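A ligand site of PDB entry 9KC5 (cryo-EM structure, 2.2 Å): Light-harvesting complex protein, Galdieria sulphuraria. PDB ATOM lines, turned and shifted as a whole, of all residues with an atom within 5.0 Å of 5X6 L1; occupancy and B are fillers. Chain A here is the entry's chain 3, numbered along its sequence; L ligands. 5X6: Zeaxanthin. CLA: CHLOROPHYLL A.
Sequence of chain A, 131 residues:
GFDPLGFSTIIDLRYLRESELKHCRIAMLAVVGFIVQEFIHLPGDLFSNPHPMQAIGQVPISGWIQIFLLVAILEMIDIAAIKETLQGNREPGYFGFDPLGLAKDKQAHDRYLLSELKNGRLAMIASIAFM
An oxygen (O37) of 5X6 L1 lies within hydrogen-bond range of the side-chain carboxylate of Asp 3 (2.7 Å). N of Leu 5 is in hydrogen-bond range of O37 of 5X6 L1 (3.0 Å). A ring nitrogen (NE2) of His 23 is bound to a magnesium atom (MG) of CLA L2 (2.5 Å). N of Phe 2 sits at hydrogen-bond distance from OBD of CLA L3 (3.1 Å).
The backbone NH of Gly 6 lies within hydrogen-bond range of the side-chain carboxylate of Asp 3 (2.9 Å). The backbone NH of Phe 7 sits at hydrogen-bond distance from the side-chain carboxylate of Asp 3 (3.1 Å). The side-chain hydroxyl (OG) of Ser 127 lies within hydrogen-bond range of the backbone carbonyl oxygen (O) of Met 124, at 2.7 Å. O of Ile 56 sits at hydrogen-bond distance from NE1 of Trp 64, at 3.1 Å.
N of Pro 4 lies close to O37 of 5X6 L1, at 3.4 Å. Phe 2 touches 5X6 L1 (CZ to C35, 3.8 Å). Gly 6 touches 5X6 L1 (N to O37, 3.9 Å). His 23 touches 5X6 L1. CG2 of Ile 26 touches C41 of 5X6 L1, 3.999 Å away. CB of Ala 27 touches C18 of 5X6 L1, 3.8 Å away. CB of Ala 30 touches C14 of 5X6 L1 (3.4 Å). Phe 34 touches 5X6 L1. CB of Ala 55 touches O08 of 5X6 L1 (3.9 Å). Ile 56 touches 5X6 L1 (CD1 to C09, 3.9 Å). CH2 of Trp 64 touches C10 of 5X6 L1, 3.9 Å away. Met 124 touches 5X6 L1 (O to C20, 3.4 Å). Ile 125 touches 5X6 L1. Ser 127 touches 5X6 L1. Ile 128 touches 5X6 L1 (CD1 to C40, 3.4 Å). Met 131 touches 5X6 L1. Within 4 Å of 5X6 L1: Phe 2, Asp 3, Pro 4, Leu 5, Gly 6, His 23, Ile 26, Ala 27, Ala 30, Phe 34, Ala 55, Ile 56, Trp 64, Met 124, Ile 125, Ser 127, Ile 128 and Met 131. The nearest printed residue that does not touch 5X6 L1 is Phe 7 (4.4 Å).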
ATOM      1  N   PHE A   2      10.495   0.728  -5.563  1.00  0.00           N
ATOM      2  CA  PHE A   2      11.248   1.861  -6.065  1.00  0.00           C
ATOM      3  C   PHE A   2      10.789   2.165  -7.499  1.00  0.00           C
ATOM      4  O   PHE A   2      11.311   1.595  -8.457  1.00  0.00           O
ATOM      5  CB  PHE A   2      12.741   1.547  -5.959  1.00  0.00           C
ATOM      6  CG  PHE A   2      13.684   2.608  -6.509  1.00  0.00           C
ATOM      7  CD1 PHE A   2      13.764   3.860  -5.912  1.00  0.00           C
ATOM      8  CD2 PHE A   2      14.528   2.342  -7.589  1.00  0.00           C
ATOM      9  CE1 PHE A   2      14.626   4.833  -6.405  1.00  0.00           C
ATOM     10  CE2 PHE A   2      15.394   3.316  -8.069  1.00  0.00           C
ATOM     11  CZ  PHE A   2      15.442   4.553  -7.483  1.00  0.00           C
ATOM     12  N   ASP A   3       9.796   3.054  -7.619  1.00  0.00           N
ATOM     13  CA  ASP A   3       9.346   3.568  -8.903  1.00  0.00           C
ATOM     14  C   ASP A   3       8.911   5.021  -8.740  1.00  0.00           C
ATOM     15  O   ASP A   3       7.721   5.314  -8.778  1.00  0.00           O
ATOM     16  CB  ASP A   3       8.250   2.676  -9.477  1.00  0.00           C
ATOM     17  CG  ASP A   3       7.902   2.909 -10.937  1.00  0.00           C
ATOM     18  OD1 ASP A   3       8.591   3.719 -11.597  1.00  0.00           O
ATOM     19  OD2 ASP A   3       6.930   2.279 -11.415  1.00  0.00           O
ATOM     20  N   PRO A   4       9.852   5.964  -8.541  1.00  0.00           N
ATOM     21  CA  PRO A   4       9.534   7.397  -8.523  1.00  0.00           C
ATOM     22  C   PRO A   4       8.771   7.907  -9.750  1.00  0.00           C
ATOM     23  O   PRO A   4       7.753   8.585  -9.601  1.00  0.00           O
ATOM     24  CB  PRO A   4      10.893   8.076  -8.417  1.00  0.00           C
ATOM     25  CG  PRO A   4      11.781   7.022  -7.773  1.00  0.00           C
ATOM     26  CD  PRO A   4      11.273   5.703  -8.249  1.00  0.00           C
ATOM     27  N   LEU A   5       9.271   7.577 -10.951  1.00  0.00           N
ATOM     28  CA  LEU A   5       8.754   8.122 -12.189  1.00  0.00           C
ATOM     29  C   LEU A   5       7.385   7.513 -12.514  1.00  0.00           C
ATOM     30  O   LEU A   5       6.475   8.232 -12.921  1.00  0.00           O
ATOM     31  CB  LEU A   5       9.757   7.907 -13.322  1.00  0.00           C
ATOM     32  CG  LEU A   5      11.092   8.644 -13.179  1.00  0.00           C
ATOM     33  CD1 LEU A   5      12.122   8.145 -14.190  1.00  0.00           C
ATOM     34  CD2 LEU A   5      10.933  10.143 -13.319  1.00  0.00           C
ATOM     35  N   GLY A   6       7.263   6.192 -12.349  1.00  0.00           N
ATOM     36  CA  GLY A   6       5.984   5.506 -12.448  1.00  0.00           C
ATOM     37  C   GLY A   6       5.816   4.808 -13.794  1.00  0.00           C
ATOM     38  O   GLY A   6       4.808   5.020 -14.477  1.00  0.00           O
ATOM     39  N   PHE A   7       6.796   3.968 -14.158  1.00  0.00           N
ATOM     40  CA  PHE A   7       6.772   3.220 -15.401  1.00  0.00           C
ATOM     41  C   PHE A   7       5.905   1.963 -15.252  1.00  0.00           C
ATOM     42  O   PHE A   7       5.327   1.499 -16.237  1.00  0.00           O
ATOM     43  CB  PHE A   7       8.197   2.867 -15.834  1.00  0.00           C
ATOM     44  CG  PHE A   7       8.934   3.988 -16.545  1.00  0.00           C
ATOM     45  CD1 PHE A   7       9.460   5.066 -15.838  1.00  0.00           C
ATOM     46  CD2 PHE A   7       9.112   3.960 -17.930  1.00  0.00           C
ATOM     47  CE1 PHE A   7      10.126   6.089 -16.494  1.00  0.00           C
ATOM     48  CE2 PHE A   7       9.791   4.986 -18.583  1.00  0.00           C
ATOM     49  CZ  PHE A   7      10.296   6.044 -17.867  1.00  0.00           C
ATOM     50  N   HIS A  23      18.813  -6.931 -19.411  1.00  0.00           N
ATOM     51  CA  HIS A  23      19.889  -5.991 -19.163  1.00  0.00           C
ATOM     52  C   HIS A  23      20.892  -6.570 -18.169  1.00  0.00           C
ATOM     53  O   HIS A  23      22.103  -6.465 -18.369  1.00  0.00           O
ATOM     54  CB  HIS A  23      19.367  -4.644 -18.651  1.00  0.00           C
ATOM     55  CG  HIS A  23      18.874  -3.702 -19.696  1.00  0.00           C
ATOM     56  ND1 HIS A  23      17.549  -3.623 -20.099  1.00  0.00           N
ATOM     57  CD2 HIS A  23      19.523  -2.778 -20.410  1.00  0.00           C
ATOM     58  CE1 HIS A  23      17.432  -2.683 -21.026  1.00  0.00           C
ATOM     59  NE2 HIS A  23      18.620  -2.155 -21.231  1.00  0.00           N
ATOM     60  N   ILE A  26      22.939  -9.517 -19.921  1.00  0.00           N
ATOM     61  CA  ILE A  26      23.830  -8.997 -20.957  1.00  0.00           C
ATOM     62  C   ILE A  26      24.992  -8.247 -20.296  1.00  0.00           C
ATOM     63  O   ILE A  26      26.138  -8.411 -20.713  1.00  0.00           O
ATOM     64  CB  ILE A  26      23.068  -8.096 -21.955  1.00  0.00           C
ATOM     65  CG1 ILE A  26      22.065  -8.910 -22.788  1.00  0.00           C
ATOM     66  CG2 ILE A  26      24.039  -7.328 -22.857  1.00  0.00           C
ATOM     67  CD1 ILE A  26      21.003  -8.068 -23.468  1.00  0.00           C
ATOM     68  N   ALA A  27      24.671  -7.437 -19.278  1.00  0.00           N
ATOM     69  CA  ALA A  27      25.665  -6.618 -18.598  1.00  0.00           C
ATOM     70  C   ALA A  27      26.709  -7.489 -17.887  1.00  0.00           C
ATOM     71  O   ALA A  27      27.902  -7.190 -17.971  1.00  0.00           O
ATOM     72  CB  ALA A  27      24.984  -5.681 -17.621  1.00  0.00           C
ATOM     73  N   ALA A  30      29.056  -9.148 -20.143  1.00  0.00           N
ATOM     74  CA  ALA A  30      29.941  -8.101 -20.621  1.00  0.00           C
ATOM     75  C   ALA A  30      31.008  -7.759 -19.582  1.00  0.00           C
ATOM     76  O   ALA A  30      32.174  -7.635 -19.919  1.00  0.00           O
ATOM     77  CB  ALA A  30      29.140  -6.878 -21.014  1.00  0.00           C
ATOM     78  N   GLY A  33      33.237 -10.396 -19.679  1.00  0.00           N
ATOM     79  CA  GLY A  33      33.868 -10.297 -20.983  1.00  0.00           C
ATOM     80  C   GLY A  33      34.948  -9.224 -21.056  1.00  0.00           C
ATOM     81  O   GLY A  33      35.999  -9.444 -21.661  1.00  0.00           O
ATOM     82  N   PHE A  34      34.678  -8.060 -20.442  1.00  0.00           N
ATOM     83  CA  PHE A  34      35.631  -6.952 -20.399  1.00  0.00           C
ATOM     84  C   PHE A  34      36.902  -7.360 -19.652  1.00  0.00           C
ATOM     85  O   PHE A  34      37.999  -7.037 -20.096  1.00  0.00           O
ATOM     86  CB  PHE A  34      35.014  -5.721 -19.719  1.00  0.00           C
ATOM     87  CG  PHE A  34      33.963  -4.949 -20.498  1.00  0.00           C
ATOM     88  CD1 PHE A  34      34.200  -4.532 -21.811  1.00  0.00           C
ATOM     89  CD2 PHE A  34      32.738  -4.631 -19.927  1.00  0.00           C
ATOM     90  CE1 PHE A  34      33.237  -3.826 -22.519  1.00  0.00           C
ATOM     91  CE2 PHE A  34      31.776  -3.924 -20.636  1.00  0.00           C
ATOM     92  CZ  PHE A  34      32.032  -3.521 -21.930  1.00  0.00           C
ATOM     93  N   MET A  53      37.542  -2.523 -27.016  1.00  0.00           N
ATOM     94  CA  MET A  53      37.350  -1.479 -28.066  1.00  0.00           C
ATOM     95  C   MET A  53      38.042  -1.920 -29.362  1.00  0.00           C
ATOM     96  O   MET A  53      37.455  -1.826 -30.431  1.00  0.00           O
ATOM     97  CB  MET A  53      37.920  -0.119 -27.626  1.00  0.00           C
ATOM     98  CG  MET A  53      37.665   0.226 -26.166  1.00  0.00           C
ATOM     99  SD  MET A  53      38.831  -0.569 -25.048  1.00  0.00           S
ATOM    100  CE  MET A  53      40.351   0.325 -25.423  1.00  0.00           C
ATOM    101  N   ALA A  55      38.958  -5.039 -29.951  1.00  0.00           N
ATOM    102  CA  ALA A  55      38.356  -6.322 -30.263  1.00  0.00           C
ATOM    103  C   ALA A  55      37.086  -6.173 -31.106  1.00  0.00           C
ATOM    104  O   ALA A  55      36.678  -7.127 -31.766  1.00  0.00           O
ATOM    105  CB  ALA A  55      38.070  -7.069 -28.980  1.00  0.00           C
ATOM    106  N   ILE A  56      36.446  -4.994 -31.059  1.00  0.00           N
ATOM    107  CA  ILE A  56      35.304  -4.694 -31.913  1.00  0.00           C
ATOM    108  C   ILE A  56      35.765  -4.682 -33.379  1.00  0.00           C
ATOM    109  O   ILE A  56      35.035  -5.132 -34.253  1.00  0.00           O
ATOM    110  CB  ILE A  56      34.615  -3.372 -31.519  1.00  0.00           C
ATOM    111  CG1 ILE A  56      34.207  -3.341 -30.030  1.00  0.00           C
ATOM    112  CG2 ILE A  56      33.405  -3.096 -32.417  1.00  0.00           C
ATOM    113  CD1 ILE A  56      33.849  -1.957 -29.518  1.00  0.00           C
ATOM    114  N   TRP A  64      31.439 -11.807 -36.369  1.00  0.00           N
ATOM    115  CA  TRP A  64      30.521 -10.842 -35.777  1.00  0.00           C
ATOM    116  C   TRP A  64      29.091 -11.036 -36.288  1.00  0.00           C
ATOM    117  O   TRP A  64      28.129 -10.835 -35.544  1.00  0.00           O
ATOM    118  CB  TRP A  64      30.992  -9.403 -36.037  1.00  0.00           C
ATOM    119  CG  TRP A  64      31.795  -8.773 -34.923  1.00  0.00           C
ATOM    120  CD1 TRP A  64      33.098  -8.365 -34.977  1.00  0.00           C
ATOM    121  CD2 TRP A  64      31.341  -8.480 -33.583  1.00  0.00           C
ATOM    122  NE1 TRP A  64      33.485  -7.832 -33.781  1.00  0.00           N
ATOM    123  CE2 TRP A  64      32.432  -7.888 -32.899  1.00  0.00           C
ATOM    124  CE3 TRP A  64      30.135  -8.651 -32.887  1.00  0.00           C
ATOM    125  CZ2 TRP A  64      32.347  -7.480 -31.578  1.00  0.00           C
ATOM    126  CZ3 TRP A  64      30.053  -8.238 -31.583  1.00  0.00           C
ATOM    127  CH2 TRP A  64      31.146  -7.660 -30.926  1.00  0.00           C
ATOM    128  N   MET A 124      25.303  -3.818 -14.220  1.00  0.00           N
ATOM    129  CA  MET A 124      24.808  -2.884 -15.219  1.00  0.00           C
ATOM    130  C   MET A 124      25.423  -1.497 -15.027  1.00  0.00           C
ATOM    131  O   MET A 124      25.830  -0.869 -15.998  1.00  0.00           O
ATOM    132  CB  MET A 124      23.271  -2.801 -15.152  1.00  0.00           C
ATOM    133  CG  MET A 124      22.586  -4.012 -15.752  1.00  0.00           C
ATOM    134  SD  MET A 124      20.920  -4.262 -15.111  1.00  0.00           S
ATOM    135  CE  MET A 124      20.151  -2.744 -15.666  1.00  0.00           C
ATOM    136  N   ILE A 125      25.484  -1.029 -13.770  1.00  0.00           N
ATOM    137  CA  ILE A 125      26.113   0.236 -13.434  1.00  0.00           C
ATOM    138  C   ILE A 125      27.621   0.124 -13.675  1.00  0.00           C
ATOM    139  O   ILE A 125      28.242   1.082 -14.132  1.00  0.00           O
ATOM    140  CB  ILE A 125      25.770   0.657 -11.986  1.00  0.00           C
ATOM    141  CG1 ILE A 125      24.284   0.980 -11.843  1.00  0.00           C
ATOM    142  CG2 ILE A 125      26.648   1.829 -11.528  1.00  0.00           C
ATOM    143  CD1 ILE A 125      23.793   1.077 -10.410  1.00  0.00           C
ATOM    144  N   SER A 127      29.104  -1.883 -15.880  1.00  0.00           N
ATOM    145  CA  SER A 127      29.363  -2.050 -17.310  1.00  0.00           C
ATOM    146  C   SER A 127      29.425  -0.704 -18.024  1.00  0.00           C
ATOM    147  O   SER A 127      30.172  -0.570 -18.996  1.00  0.00           O
ATOM    148  CB  SER A 127      28.348  -2.960 -17.936  1.00  0.00           C
ATOM    149  OG  SER A 127      27.034  -2.445 -17.769  1.00  0.00           O
ATOM    150  N   ILE A 128      28.625   0.271 -17.573  1.00  0.00           N
ATOM    151  CA  ILE A 128      28.647   1.626 -18.121  1.00  0.00           C
ATOM    152  C   ILE A 128      30.030   2.241 -17.889  1.00  0.00           C
ATOM    153  O   ILE A 128      30.590   2.834 -18.806  1.00  0.00           O
ATOM    154  CB  ILE A 128      27.527   2.491 -17.518  1.00  0.00           C
ATOM    155  CG1 ILE A 128      26.144   2.016 -17.958  1.00  0.00           C
ATOM    156  CG2 ILE A 128      27.735   3.974 -17.839  1.00  0.00           C
ATOM    157  CD1 ILE A 128      24.995   2.613 -17.160  1.00  0.00           C
ATOM    158  N   MET A 131      32.701   0.772 -20.173  1.00  0.00           N
ATOM    159  CA  MET A 131      32.505   1.326 -21.507  1.00  0.00           C
ATOM    160  C   MET A 131      32.841   2.827 -21.504  1.00  0.00           C
ATOM    161  O   MET A 131      33.289   3.307 -22.568  1.00  0.00           O
ATOM    162  CB  MET A 131      31.051   1.144 -21.983  1.00  0.00           C
ATOM    163  CG  MET A 131      30.699  -0.278 -22.376  1.00  0.00           C
ATOM    164  SD  MET A 131      29.042  -0.428 -23.069  1.00  0.00           S
ATOM    165  CE  MET A 131      28.004   0.042 -21.688  1.00  0.00           C
HETATM  166  C17 5X6 L   1      24.442  -2.840 -20.577  1.00  0.00           C
HETATM  167  C18 5X6 L   1      24.189  -2.339 -19.283  1.00  0.00           C
HETATM  168  C16 5X6 L   1      25.862  -3.427 -20.714  1.00  0.00           C
HETATM  169  C26 5X6 L   1      18.210   2.619 -13.549  1.00  0.00           C
HETATM  170  C19 5X6 L   1      23.181  -1.155 -19.261  1.00  0.00           C
HETATM  171  C10 5X6 L   1      30.275  -5.521 -27.776  1.00  0.00           C
HETATM  172  C11 5X6 L   1      30.209  -4.637 -24.579  1.00  0.00           C
HETATM  173  C12 5X6 L   1      29.065  -5.156 -24.032  1.00  0.00           C
HETATM  174  C13 5X6 L   1      28.012  -4.068 -23.667  1.00  0.00           C
HETATM  175  C20 5X6 L   1      23.025  -0.654 -17.974  1.00  0.00           C
HETATM  176  C14 5X6 L   1      27.439  -4.273 -22.390  1.00  0.00           C
HETATM  177  C15 5X6 L   1      26.452  -3.159 -21.944  1.00  0.00           C
HETATM  178  C35 5X6 L   1      15.639   6.146 -10.929  1.00  0.00           C
HETATM  179  C34 5X6 L   1      14.710   5.428 -11.922  1.00  0.00           C
HETATM  180  C33 5X6 L   1      13.220   5.787 -11.529  1.00  0.00           C
HETATM  181  C40 5X6 L   1      22.599   0.951 -15.503  1.00  0.00           C
HETATM  182  C32 5X6 L   1      12.164   4.835 -12.175  1.00  0.00           C
HETATM  183  C31 5X6 L   1      12.493   3.373 -11.845  1.00  0.00           C
HETATM  184  C30 5X6 L   1      13.933   3.000 -12.043  1.00  0.00           C
HETATM  185  C29 5X6 L   1      14.905   3.913 -11.835  1.00  0.00           C
HETATM  186  C39 5X6 L   1      19.242   3.449 -12.785  1.00  0.00           C
HETATM  187  C28 5X6 L   1      16.385   3.419 -12.068  1.00  0.00           C
HETATM  188  C27 5X6 L   1      16.711   3.044 -13.346  1.00  0.00           C
HETATM  189  C21 5X6 L   1      21.756   0.214 -17.772  1.00  0.00           C
HETATM  190  C36 5X6 L   1      14.961   5.956 -13.333  1.00  0.00           C
HETATM  191  C22 5X6 L   1      21.435   0.645 -16.458  1.00  0.00           C
HETATM  192  C23 5X6 L   1      20.290   1.690 -16.491  1.00  0.00           C
HETATM  193  C24 5X6 L   1      20.002   2.376 -15.320  1.00  0.00           C
HETATM  194  C25 5X6 L   1      18.501   2.396 -14.922  1.00  0.00           C
HETATM  195  C38 5X6 L   1      14.196   1.663 -11.344  1.00  0.00           C
HETATM  196  C01 5X6 L   1      31.507  -7.581 -24.135  1.00  0.00           C
HETATM  197  C02 5X6 L   1      31.993  -6.217 -24.636  1.00  0.00           C
HETATM  198  C03 5X6 L   1      31.076  -5.622 -25.412  1.00  0.00           C
HETATM  199  C04 5X6 L   1      31.382  -5.086 -26.811  1.00  0.00           C
HETATM  200  C05 5X6 L   1      32.726  -5.723 -27.321  1.00  0.00           C
HETATM  201  C06 5X6 L   1      33.871  -5.598 -26.265  1.00  0.00           C
HETATM  202  C07 5X6 L   1      33.453  -6.351 -25.009  1.00  0.00           C
HETATM  203  O08 5X6 L   1      35.032  -6.141 -26.769  1.00  0.00           O
HETATM  204  C09 5X6 L   1      31.516  -3.552 -26.879  1.00  0.00           C
HETATM  205  O37 5X6 L   1      10.910   5.132 -11.690  1.00  0.00           O
HETATM  206  C41 5X6 L   1      23.360  -3.818 -21.064  1.00  0.00           C
HETATM  207  C42 5X6 L   1      26.999  -3.862 -24.800  1.00  0.00           C
HETATM  208 MG   CLA L   2      18.811  -0.068 -22.677  1.00  0.00          MG
HETATM  209  CHA CLA L   2      15.711  -0.678 -24.070  1.00  0.00           C
HETATM  210  CHB CLA L   2      17.286   1.994 -20.452  1.00  0.00           C
HETATM  211  CHC CLA L   2      21.910   0.933 -21.736  1.00  0.00           C
HETATM  212  CHD CLA L   2      20.311  -1.997 -25.474  1.00  0.00           C
HETATM  213  NA  CLA L   2      16.859   0.575 -22.329  1.00  0.00           N
HETATM  214  C1A CLA L   2      15.761   0.160 -22.839  1.00  0.00           C
HETATM  215  C2A CLA L   2      14.476   0.612 -22.183  1.00  0.00           C
HETATM  216  C3A CLA L   2      15.017   1.495 -21.072  1.00  0.00           C
HETATM  217  C4A CLA L   2      16.492   1.345 -21.307  1.00  0.00           C
HETATM  218  CMA CLA L   2      14.523   2.929 -21.276  1.00  0.00           C
HETATM  219  CAA CLA L   2      13.697  -0.558 -21.581  1.00  0.00           C
HETATM  220  CBA CLA L   2      12.335  -0.152 -21.009  1.00  0.00           C
HETATM  221  CGA CLA L   2      11.318   0.027 -22.108  1.00  0.00           C
HETATM  222  O1A CLA L   2      10.983  -0.915 -22.806  1.00  0.00           O
HETATM  223  O2A CLA L   2      10.702   1.322 -22.334  1.00  0.00           O
HETATM  224  NB  CLA L   2      19.493   1.242 -21.264  1.00  0.00           N
HETATM  225  C1B CLA L   2      18.759   2.007 -20.459  1.00  0.00           C
HETATM  226  C2B CLA L   2      19.541   2.936 -19.595  1.00  0.00           C
HETATM  227  C3B CLA L   2      20.943   2.613 -19.981  1.00  0.00           C
HETATM  228  C4B CLA L   2      20.770   1.548 -21.017  1.00  0.00           C
HETATM  229  CMB CLA L   2      18.980   3.919 -18.600  1.00  0.00           C
HETATM  230  CAB CLA L   2      22.266   3.167 -19.546  1.00  0.00           C
HETATM  231  CBB CLA L   2      22.402   4.215 -18.750  1.00  0.00           C
HETATM  232  NC  CLA L   2      20.687  -0.433 -23.465  1.00  0.00           N
HETATM  233  C1C CLA L   2      21.814   0.026 -22.887  1.00  0.00           C
HETATM  234  C2C CLA L   2      23.079  -0.434 -23.543  1.00  0.00           C
HETATM  235  C3C CLA L   2      22.597  -1.297 -24.637  1.00  0.00           C
HETATM  236  C4C CLA L   2      21.119  -1.231 -24.496  1.00  0.00           C
HETATM  237  CMC CLA L   2      24.499  -0.106 -23.170  1.00  0.00           C
HETATM  238  CAC CLA L   2      23.419  -2.069 -25.660  1.00  0.00           C
HETATM  239  CBC CLA L   2      23.422  -3.517 -25.227  1.00  0.00           C
HETATM  240  ND  CLA L   2      18.261  -1.096 -24.355  1.00  0.00           N
HETATM  241  C1D CLA L   2      18.852  -1.842 -25.438  1.00  0.00           C
HETATM  242  C2D CLA L   2      17.902  -2.378 -26.453  1.00  0.00           C
HETATM  243  C3D CLA L   2      16.635  -1.872 -25.876  1.00  0.00           C
HETATM  244  C4D CLA L   2      16.933  -1.166 -24.718  1.00  0.00           C
HETATM  245  CMD CLA L   2      17.994  -3.172 -27.725  1.00  0.00           C
HETATM  246  CAD CLA L   2      15.157  -1.817 -26.046  1.00  0.00           C
HETATM  247  OBD CLA L   2      14.529  -2.362 -27.021  1.00  0.00           O
HETATM  248  CBD CLA L   2      14.555  -1.046 -24.932  1.00  0.00           C
HETATM  249  CGD CLA L   2      13.867   0.167 -25.491  1.00  0.00           C
HETATM  250  O1D CLA L   2      14.460   0.967 -26.204  1.00  0.00           O
HETATM  251  O2D CLA L   2      12.462   0.406 -25.199  1.00  0.00           O
HETATM  252  CED CLA L   2      11.603   0.951 -26.194  1.00  0.00           C
HETATM  253 MG   CLA L   3      15.025  -1.801 -11.882  1.00  0.00          MG
HETATM  254  CHA CLA L   3      12.363  -2.152  -9.688  1.00  0.00           C
HETATM  255  CHB CLA L   3      12.857  -2.345 -14.434  1.00  0.00           C
HETATM  256  CHC CLA L   3      17.566  -1.013 -13.979  1.00  0.00           C
HETATM  257  CHD CLA L   3      17.124  -0.887  -8.973  1.00  0.00           C
HETATM  258  NA  CLA L   3      12.989  -2.143 -12.056  1.00  0.00           N
HETATM  259  C1A CLA L   3      12.099  -2.316 -11.142  1.00  0.00           C
HETATM  260  C2A CLA L   3      10.708  -2.653 -11.603  1.00  0.00           C
HETATM  261  C3A CLA L   3      10.903  -2.792 -13.092  1.00  0.00           C
HETATM  262  C4A CLA L   3      12.353  -2.399 -13.203  1.00  0.00           C
HETATM  263  CMA CLA L   3      10.702  -4.264 -13.472  1.00  0.00           C
HETATM  264  CAA CLA L   3       9.720  -1.506 -11.331  1.00  0.00           C
HETATM  265  CBA CLA L   3      10.254  -0.071 -11.513  1.00  0.00           C
HETATM  266  CGA CLA L   3      10.306   0.365 -12.959  1.00  0.00           C
HETATM  267  O1A CLA L   3       9.277   0.533 -13.586  1.00  0.00           O
HETATM  268  O2A CLA L   3      11.585   0.595 -13.624  1.00  0.00           O
HETATM  269  NB  CLA L   3      15.187  -1.683 -13.925  1.00  0.00           N
HETATM  270  C1B CLA L   3      14.233  -1.999 -14.800  1.00  0.00           C
HETATM  271  C2B CLA L   3      14.633  -1.932 -16.225  1.00  0.00           C
HETATM  272  C3B CLA L   3      16.058  -1.532 -16.136  1.00  0.00           C
HETATM  273  C4B CLA L   3      16.294  -1.398 -14.641  1.00  0.00           C
HETATM  274  CMB CLA L   3      13.800  -2.224 -17.451  1.00  0.00           C
HETATM  275  CAB CLA L   3      16.901  -1.329 -17.344  1.00  0.00           C
HETATM  276  CBB CLA L   3      18.135  -0.870 -17.384  1.00  0.00           C
HETATM  277  NC  CLA L   3      16.908  -1.043 -11.525  1.00  0.00           N
HETATM  278  C1C CLA L   3      17.811  -0.875 -12.524  1.00  0.00           C
HETATM  279  C2C CLA L   3      19.183  -0.550 -12.033  1.00  0.00           C
HETATM  280  C3C CLA L   3      19.045  -0.517 -10.572  1.00  0.00           C
HETATM  281  C4C CLA L   3      17.608  -0.837 -10.369  1.00  0.00           C
HETATM  282  CMC CLA L   3      20.448  -0.307 -12.807  1.00  0.00           C
HETATM  283  CAC CLA L   3      20.114  -0.239  -9.533  1.00  0.00           C
HETATM  284  CBC CLA L   3      19.934   1.194  -9.065  1.00  0.00           C
HETATM  285  ND  CLA L   3      14.885  -1.520  -9.862  1.00  0.00           N
HETATM  286  C1D CLA L   3      15.726  -1.234  -8.735  1.00  0.00           C
HETATM  287  C2D CLA L   3      15.077  -1.315  -7.398  1.00  0.00           C
HETATM  288  C3D CLA L   3      13.695  -1.689  -7.814  1.00  0.00           C
HETATM  289  C4D CLA L   3      13.698  -1.773  -9.200  1.00  0.00           C
HETATM  290  CMD CLA L   3      15.487  -1.117  -5.962  1.00  0.00           C
HETATM  291  CAD CLA L   3      12.319  -2.003  -7.340  1.00  0.00           C
HETATM  292  OBD CLA L   3      11.942  -2.013  -6.115  1.00  0.00           O
HETATM  293  CBD CLA L   3      11.454  -2.302  -8.519  1.00  0.00           C
HETATM  294  CGD CLA L   3      10.923  -3.707  -8.400  1.00  0.00           C
HETATM  295  O1D CLA L   3       9.730  -3.925  -8.556  1.00  0.00           O
HETATM  296  O2D CLA L   3      11.807  -4.810  -8.090  1.00  0.00           O
HETATM  297  CED CLA L   3      11.709  -5.483  -6.841  1.00  0.00           C
HETATM  298  C1  CLA L   3      11.674   1.078 -14.975  1.00  0.00           C
HETATM  299  C2  CLA L   3      13.085   1.539 -15.275  1.00  0.00           C
HETATM  300  C3  CLA L   3      13.437   2.013 -16.487  1.00  0.00           C
HETATM  301  C4  CLA L   3      12.424   2.122 -17.594  1.00  0.00           C
HETATM  302  C5  CLA L   3      14.859   2.468 -16.738  1.00  0.00           C
HETATM  303  C6  CLA L   3      15.025   3.959 -16.506  1.00  0.00           C
HETATM  304  C7  CLA L   3      14.978   4.775 -17.788  1.00  0.00           C
HETATM  305  C8  CLA L   3      15.302   6.259 -17.535  1.00  0.00           C
HETATM  306  C9  CLA L   3      14.425   7.155 -18.409  1.00  0.00           C
HETATM  307  C10 CLA L   3      16.794   6.483 -17.787  1.00  0.00           C
HETATM  308  C11 CLA L   3      17.327   7.893 -17.536  1.00  0.00           C
HETATM  309  C12 CLA L   3      17.046   8.412 -16.132  1.00  0.00           C
HETATM  310  C13 CLA L   3      18.125   9.359 -15.581  1.00  0.00           C
HETATM  311  C14 CLA L   3      18.578  10.384 -16.620  1.00  0.00           C
HETATM  312  C15 CLA L   3      19.285   8.550 -15.001  1.00  0.00           C
HETATM  313  C16 CLA L   3      20.436   9.368 -14.427  1.00  0.00           C
HETATM  314  C17 CLA L   3      19.987  10.371 -13.356  1.00  0.00           C
HETATM  315  C18 CLA L   3      21.064  10.724 -12.335  1.00  0.00           C
HETATM  316  C19 CLA L   3      22.422  11.018 -12.971  1.00  0.00           C
HETATM  317  C20 CLA L   3      21.194   9.652 -11.256  1.00  0.00           C
